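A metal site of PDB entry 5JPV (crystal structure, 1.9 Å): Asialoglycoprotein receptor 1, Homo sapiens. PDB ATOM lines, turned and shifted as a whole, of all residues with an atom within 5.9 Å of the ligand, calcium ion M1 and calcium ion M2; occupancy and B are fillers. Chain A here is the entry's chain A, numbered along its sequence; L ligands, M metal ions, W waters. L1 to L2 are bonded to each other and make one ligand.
The side-chain carboxylate (OD1) of Asp 97 is bound to calcium ion M2 (2.4 Å). The backbone carbonyl oxygen (O) of Glu 107 is bound to calcium ion M2. Water W3 is bound to calcium ion M2, at 2.4 Å. Calcium ion M2 is bound by water W8, 2.5 Å away. Calcium ion M2 is bound by OD1 of Asp 108 (2.6 Å). Water W6 binds calcium ion M2, 2.6 Å away. The side-chain carboxylate (OD2) of Asp 70 is bound to calcium ion M2 (2.6 Å). Calcium ion M2 is bound by the side-chain carboxylate (OD1) of Asp 70, 2.7 Å away.
The guanidinium group (NH1) of Arg 91 lies within hydrogen-bond range of an oxygen (O1) of LIG L1, 3.2 Å away.
The backbone NH (N) of Trp 98 lies close to the side-chain carboxylate (OE2) of Glu 107. The side-chain carboxylate (OD2) of Asp 120 is in hydrogen-bond range of the backbone NH (N) of Asp 97 (2.8 Å). N of Trp 98 sits close to OD1 of Asp 96. The backbone NH (N) of His 111 sits at hydrogen-bond distance from the backbone carbonyl oxygen (O) of Asn 119, 2.9 Å away. O of Asp 121 lies within hydrogen-bond range of N of Asp 108, at 3.1 Å.
Water W2 bridges an oxygen (O1) of LG2 L2 (3.3 Å) and the side-chain carboxylate of Asp 121 (3.4 Å). Water W5 lies within hydrogen-bond range of the side-chain amide nitrogen of Gln 94 (2.8 Å) and an oxygen (O3) of LIG L1 (3.3 Å).
Within 4 Å of calcium ion M2: Asp 70, Asp 97, Glu 107 and Asp 108. The nearest printed residue that does not touch calcium ion M2 is Asp 120 (4.7 Å).
Within 4 Å of calcium ion M1: Gln 94, Asp 96, Glu 107, Asn 119 and Asp 120. The nearest printed residue that does not touch calcium ion M1 is Asp 121 (4.8 Å).
Merely in contact with the ligand: Trp 98. Hydrophobic or aromatic side chains that line the ligand: Trp 98.
Calcium ion M1 is bound by OE2 of Glu 107, OD1 of Asp 120, OD1 of Asp 96, OD1 of Asn 119, O3 of LG2 L2, O of Asp 120, O2 of LG2 L2 and OE1 of Gln 94.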
ATOM      1  N   ASP A  70      11.268 -37.168  -2.882  1.00  0.00           N
ATOM      2  CA  ASP A  70      12.397 -37.609  -2.039  1.00  0.00           C
ATOM      3  C   ASP A  70      12.236 -37.143  -0.585  1.00  0.00           C
ATOM      4  O   ASP A  70      13.223 -36.830   0.099  1.00  0.00           O
ATOM      5  CB  ASP A  70      13.735 -37.140  -2.629  1.00  0.00           C
ATOM      6  CG  ASP A  70      14.054 -35.672  -2.338  1.00  0.00           C
ATOM      7  OD1 ASP A  70      13.136 -34.844  -2.178  1.00  0.00           O
ATOM      8  OD2 ASP A  70      15.245 -35.358  -2.249  1.00  0.00           O
ATOM      9  N   TRP A  75      15.060 -40.374  -4.164  1.00  0.00           N
ATOM     10  CA  TRP A  75      13.941 -40.236  -5.097  1.00  0.00           C
ATOM     11  C   TRP A  75      13.167 -41.552  -5.209  1.00  0.00           C
ATOM     12  O   TRP A  75      13.781 -42.599  -5.374  1.00  0.00           O
ATOM     13  CB  TRP A  75      14.438 -39.777  -6.465  1.00  0.00           C
ATOM     14  CG  TRP A  75      14.800 -38.341  -6.469  1.00  0.00           C
ATOM     15  CD1 TRP A  75      16.062 -37.800  -6.525  1.00  0.00           C
ATOM     16  CD2 TRP A  75      13.898 -37.237  -6.379  1.00  0.00           C
ATOM     17  NE1 TRP A  75      15.988 -36.435  -6.485  1.00  0.00           N
ATOM     18  CE2 TRP A  75      14.679 -36.057  -6.383  1.00  0.00           C
ATOM     19  CE3 TRP A  75      12.507 -37.129  -6.287  1.00  0.00           C
ATOM     20  CZ2 TRP A  75      14.102 -34.776  -6.308  1.00  0.00           C
ATOM     21  CZ3 TRP A  75      11.938 -35.854  -6.212  1.00  0.00           C
ATOM     22  CH2 TRP A  75      12.735 -34.703  -6.215  1.00  0.00           C
ATOM     23  N   ARG A  91      14.444 -30.796 -15.898  1.00  0.00           N
ATOM     24  CA  ARG A  91      14.963 -29.543 -16.472  1.00  0.00           C
ATOM     25  C   ARG A  91      16.466 -29.486 -16.224  1.00  0.00           C
ATOM     26  O   ARG A  91      16.931 -29.981 -15.184  1.00  0.00           O
ATOM     27  CB  ARG A  91      14.332 -28.326 -15.788  1.00  0.00           C
ATOM     28  CG  ARG A  91      13.077 -27.823 -16.431  1.00  0.00           C
ATOM     29  CD  ARG A  91      13.097 -26.300 -16.491  1.00  0.00           C
ATOM     30  NE  ARG A  91      11.906 -25.815 -17.195  1.00  0.00           N
ATOM     31  CZ  ARG A  91      11.699 -24.564 -17.553  1.00  0.00           C
ATOM     32  NH1 ARG A  91      12.593 -23.621 -17.307  1.00  0.00           N
ATOM     33  NH2 ARG A  91      10.569 -24.263 -18.179  1.00  0.00           N
ATOM     34  N   GLU A  93      19.745 -28.297 -14.714  1.00  0.00           N
ATOM     35  CA  GLU A  93      19.989 -27.687 -13.406  1.00  0.00           C
ATOM     36  C   GLU A  93      18.994 -28.122 -12.310  1.00  0.00           C
ATOM     37  O   GLU A  93      19.028 -27.596 -11.197  1.00  0.00           O
ATOM     38  CB  GLU A  93      20.112 -26.159 -13.497  1.00  0.00           C
ATOM     39  CG  GLU A  93      21.319 -25.702 -14.332  1.00  0.00           C
ATOM     40  CD  GLU A  93      21.720 -24.258 -14.051  1.00  0.00           C
ATOM     41  OE1 GLU A  93      22.869 -24.044 -13.586  1.00  0.00           O
ATOM     42  OE2 GLU A  93      20.893 -23.347 -14.266  1.00  0.00           O
ATOM     43  N   GLN A  94      18.143 -29.079 -12.639  1.00  0.00           N
ATOM     44  CA  GLN A  94      17.229 -29.719 -11.670  1.00  0.00           C
ATOM     45  C   GLN A  94      17.531 -31.220 -11.593  1.00  0.00           C
ATOM     46  O   GLN A  94      18.080 -31.779 -12.543  1.00  0.00           O
ATOM     47  CB  GLN A  94      15.761 -29.497 -12.058  1.00  0.00           C
ATOM     48  CG  GLN A  94      15.350 -28.023 -12.308  1.00  0.00           C
ATOM     49  CD  GLN A  94      15.525 -27.120 -11.094  1.00  0.00           C
ATOM     50  OE1 GLN A  94      15.583 -27.577  -9.962  1.00  0.00           O
ATOM     51  NE2 GLN A  94      15.576 -25.810 -11.346  1.00  0.00           N
ATOM     52  N   PRO A  95      17.212 -31.877 -10.454  1.00  0.00           N
ATOM     53  CA  PRO A  95      16.710 -31.316  -9.190  1.00  0.00           C
ATOM     54  C   PRO A  95      17.835 -30.615  -8.427  1.00  0.00           C
ATOM     55  O   PRO A  95      18.998 -30.994  -8.576  1.00  0.00           O
ATOM     56  CB  PRO A  95      16.221 -32.547  -8.411  1.00  0.00           C
ATOM     57  CG  PRO A  95      17.015 -33.697  -8.970  1.00  0.00           C
ATOM     58  CD  PRO A  95      17.371 -33.337 -10.390  1.00  0.00           C
ATOM     59  N   ASP A  96      17.498 -29.600  -7.651  1.00  0.00           N
ATOM     60  CA  ASP A  96      18.527 -28.831  -6.949  1.00  0.00           C
ATOM     61  C   ASP A  96      18.273 -28.664  -5.448  1.00  0.00           C
ATOM     62  O   ASP A  96      19.053 -28.003  -4.773  1.00  0.00           O
ATOM     63  CB  ASP A  96      18.702 -27.462  -7.616  1.00  0.00           C
ATOM     64  CG  ASP A  96      17.457 -26.582  -7.518  1.00  0.00           C
ATOM     65  OD1 ASP A  96      16.402 -27.097  -7.087  1.00  0.00           O
ATOM     66  OD2 ASP A  96      17.539 -25.390  -7.886  1.00  0.00           O
ATOM     67  N   ASP A  97      17.175 -29.234  -4.946  1.00  0.00           N
ATOM     68  CA  ASP A  97      16.800 -29.138  -3.518  1.00  0.00           C
ATOM     69  C   ASP A  97      16.950 -27.715  -2.955  1.00  0.00           C
ATOM     70  O   ASP A  97      17.594 -27.513  -1.919  1.00  0.00           O
ATOM     71  CB  ASP A  97      17.634 -30.132  -2.685  1.00  0.00           C
ATOM     72  CG  ASP A  97      17.038 -30.417  -1.311  1.00  0.00           C
ATOM     73  OD1 ASP A  97      15.808 -30.633  -1.191  1.00  0.00           O
ATOM     74  OD2 ASP A  97      17.830 -30.476  -0.334  1.00  0.00           O
ATOM     75  N   TRP A  98      16.356 -26.736  -3.637  1.00  0.00           N
ATOM     76  CA  TRP A  98      16.592 -25.331  -3.305  1.00  0.00           C
ATOM     77  C   TRP A  98      15.992 -24.953  -1.948  1.00  0.00           C
ATOM     78  O   TRP A  98      14.850 -25.275  -1.674  1.00  0.00           O
ATOM     79  CB  TRP A  98      16.033 -24.456  -4.429  1.00  0.00           C
ATOM     80  CG  TRP A  98      16.286 -22.977  -4.353  1.00  0.00           C
ATOM     81  CD1 TRP A  98      17.483 -22.338  -4.173  1.00  0.00           C
ATOM     82  CD2 TRP A  98      15.306 -21.948  -4.497  1.00  0.00           C
ATOM     83  NE1 TRP A  98      17.301 -20.974  -4.186  1.00  0.00           N
ATOM     84  CE2 TRP A  98      15.978 -20.707  -4.394  1.00  0.00           C
ATOM     85  CE3 TRP A  98      13.921 -21.958  -4.721  1.00  0.00           C
ATOM     86  CZ2 TRP A  98      15.307 -19.481  -4.476  1.00  0.00           C
ATOM     87  CZ3 TRP A  98      13.247 -20.739  -4.811  1.00  0.00           C
ATOM     88  CH2 TRP A  98      13.946 -19.509  -4.684  1.00  0.00           C
ATOM     89  N   GLY A 106      14.212 -27.941   1.870  1.00  0.00           N
ATOM     90  CA  GLY A 106      14.607 -27.783   0.471  1.00  0.00           C
ATOM     91  C   GLY A 106      13.387 -27.956  -0.429  1.00  0.00           C
ATOM     92  O   GLY A 106      12.371 -27.265  -0.255  1.00  0.00           O
ATOM     93  N   GLU A 107      13.493 -28.893  -1.371  1.00  0.00           N
ATOM     94  CA  GLU A 107      12.426 -29.149  -2.328  1.00  0.00           C
ATOM     95  C   GLU A 107      12.319 -30.655  -2.505  1.00  0.00           C
ATOM     96  O   GLU A 107      13.300 -31.304  -2.851  1.00  0.00           O
ATOM     97  CB  GLU A 107      12.710 -28.451  -3.653  1.00  0.00           C
ATOM     98  CG  GLU A 107      12.567 -26.924  -3.584  1.00  0.00           C
ATOM     99  CD  GLU A 107      12.893 -26.238  -4.907  1.00  0.00           C
ATOM    100  OE1 GLU A 107      12.241 -25.209  -5.217  1.00  0.00           O
ATOM    101  OE2 GLU A 107      13.789 -26.723  -5.628  1.00  0.00           O
ATOM    102  N   ASP A 108      11.143 -31.214  -2.226  1.00  0.00           N
ATOM    103  CA  ASP A 108      11.040 -32.660  -2.128  1.00  0.00           C
ATOM    104  C   ASP A 108      10.049 -33.327  -3.093  1.00  0.00           C
ATOM    105  O   ASP A 108       9.917 -34.545  -3.073  1.00  0.00           O
ATOM    106  CB  ASP A 108      10.720 -33.072  -0.685  1.00  0.00           C
ATOM    107  CG  ASP A 108      11.872 -32.799   0.296  1.00  0.00           C
ATOM    108  OD1 ASP A 108      12.955 -32.330  -0.140  1.00  0.00           O
ATOM    109  OD2 ASP A 108      11.683 -33.061   1.499  1.00  0.00           O
ATOM    110  N   HIS A 111       7.366 -31.919 -10.163  1.00  0.00           N
ATOM    111  CA  HIS A 111       6.274 -31.532 -11.052  1.00  0.00           C
ATOM    112  C   HIS A 111       6.776 -31.276 -12.464  1.00  0.00           C
ATOM    113  O   HIS A 111       7.928 -30.917 -12.661  1.00  0.00           O
ATOM    114  CB  HIS A 111       5.538 -30.284 -10.522  1.00  0.00           C
ATOM    115  CG  HIS A 111       6.391 -29.051 -10.468  1.00  0.00           C
ATOM    116  ND1 HIS A 111       6.313 -28.042 -11.417  1.00  0.00           N
ATOM    117  CD2 HIS A 111       7.326 -28.657  -9.569  1.00  0.00           C
ATOM    118  CE1 HIS A 111       7.176 -27.085 -11.094  1.00  0.00           C
ATOM    119  NE2 HIS A 111       7.794 -27.429  -9.982  1.00  0.00           N
ATOM    120  N   ASN A 119      10.852 -30.354 -12.428  1.00  0.00           N
ATOM    121  CA  ASN A 119      11.506 -29.586 -11.393  1.00  0.00           C
ATOM    122  C   ASN A 119      11.114 -30.155 -10.018  1.00  0.00           C
ATOM    123  O   ASN A 119       9.983 -30.625  -9.867  1.00  0.00           O
ATOM    124  CB  ASN A 119      11.061 -28.130 -11.467  1.00  0.00           C
ATOM    125  CG  ASN A 119      11.627 -27.307 -10.343  1.00  0.00           C
ATOM    126  OD1 ASN A 119      12.796 -27.420 -10.025  1.00  0.00           O
ATOM    127  ND2 ASN A 119      10.783 -26.478  -9.714  1.00  0.00           N
ATOM    128  N   ASP A 120      12.029 -30.111  -9.054  1.00  0.00           N
ATOM    129  CA  ASP A 120      11.674 -30.386  -7.665  1.00  0.00           C
ATOM    130  C   ASP A 120      11.232 -29.096  -6.991  1.00  0.00           C
ATOM    131  O   ASP A 120      11.843 -28.047  -7.189  1.00  0.00           O
ATOM    132  CB  ASP A 120      12.809 -31.082  -6.879  1.00  0.00           C
ATOM    133  CG  ASP A 120      14.114 -30.284  -6.835  1.00  0.00           C
ATOM    134  OD1 ASP A 120      14.418 -29.513  -7.764  1.00  0.00           O
ATOM    135  OD2 ASP A 120      14.856 -30.465  -5.857  1.00  0.00           O
ATOM    136  N   ASP A 121      10.152 -29.158  -6.233  1.00  0.00           N
ATOM    137  CA  ASP A 121       9.597 -27.961  -5.632  1.00  0.00           C
ATOM    138  C   ASP A 121       9.099 -28.246  -4.226  1.00  0.00           C
ATOM    139  O   ASP A 121       9.132 -29.389  -3.764  1.00  0.00           O
ATOM    140  CB  ASP A 121       8.465 -27.389  -6.499  1.00  0.00           C
ATOM    141  CG  ASP A 121       8.366 -25.867  -6.421  1.00  0.00           C
ATOM    142  OD1 ASP A 121       8.036 -25.234  -7.454  1.00  0.00           O
ATOM    143  OD2 ASP A 121       8.651 -25.287  -5.351  1.00  0.00           O
HETATM  144  C1  LIG L   1      13.297 -19.776 -14.976  1.00  0.00           C
HETATM  145  C2  LIG L   1      14.658 -20.260 -14.450  1.00  0.00           C
HETATM  146  C3  LIG L   1      14.507 -21.471 -13.518  1.00  0.00           C
HETATM  147  C4  LIG L   1      13.526 -21.212 -12.376  1.00  0.00           C
HETATM  148  C5  LIG L   1      12.223 -20.577 -12.890  1.00  0.00           C
HETATM  149  C6  LIG L   1      11.479 -19.949 -11.721  1.00  0.00           C
HETATM  150  O1  LIG L   1      12.727 -20.761 -15.876  1.00  0.00           O
HETATM  151  O2  LIG L   1      15.519 -20.616 -15.544  1.00  0.00           O
HETATM  152  O3  LIG L   1      15.774 -21.827 -12.964  1.00  0.00           O
HETATM  153  O4  LIG L   1      13.295 -22.488 -11.728  1.00  0.00           O
HETATM  154  O5  LIG L   1      12.407 -19.494 -13.860  1.00  0.00           O
HETATM  155  O6  LIG L   1      10.100 -20.286 -11.829  1.00  0.00           O
HETATM  156  C1  LG2 L   2      13.393 -22.417 -10.297  1.00  0.00           C
HETATM  157  C2  LG2 L   2      12.693 -23.671  -9.779  1.00  0.00           C
HETATM  158  C3  LG2 L   2      12.918 -23.847  -8.266  1.00  0.00           C
HETATM  159  C4  LG2 L   2      14.414 -23.741  -7.914  1.00  0.00           C
HETATM  160  C5  LG2 L   2      14.974 -22.430  -8.474  1.00  0.00           C
HETATM  161  C6  LG2 L   2      16.456 -22.210  -8.182  1.00  0.00           C
HETATM  162  O1  LG2 L   2      11.289 -23.555 -10.056  1.00  0.00           O
HETATM  163  O2  LG2 L   2      12.409 -25.133  -7.868  1.00  0.00           O
HETATM  164  O3  LG2 L   2      15.091 -24.868  -8.485  1.00  0.00           O
HETATM  165  O4  LG2 L   2      14.782 -22.374  -9.918  1.00  0.00           O
HETATM  166  O5  LG2 L   2      16.771 -20.863  -8.524  1.00  0.00           O
HETATM  167 CA    CA M   1      14.090 -27.089  -7.909  1.00  0.00          CA
HETATM  168 CA    CA M   2      14.896 -32.798  -1.789  1.00  0.00          CA
HETATM  169  O   HOH W   1       7.748 -22.863 -11.672  1.00  0.00           O
HETATM  170  O   HOH W   2       9.731 -22.325  -7.444  1.00  0.00           O
HETATM  171  O   HOH W   3      15.702 -33.595   0.382  1.00  0.00           O
HETATM  172  O   HOH W   4      19.411 -20.843  -7.225  1.00  0.00           O
HETATM  173  O   HOH W   5      15.948 -24.934 -14.031  1.00  0.00           O
HETATM  174  O   HOH W   6      17.441 -33.372  -1.851  1.00  0.00           O
HETATM  175  O   HOH W   7      11.142 -24.654 -12.835  1.00  0.00           O
HETATM  176  O   HOH W   8      15.582 -32.492  -4.152  1.00  0.00           O
HETATM  177  O   HOH W   9      17.196 -20.754 -11.160  1.00  0.00           O
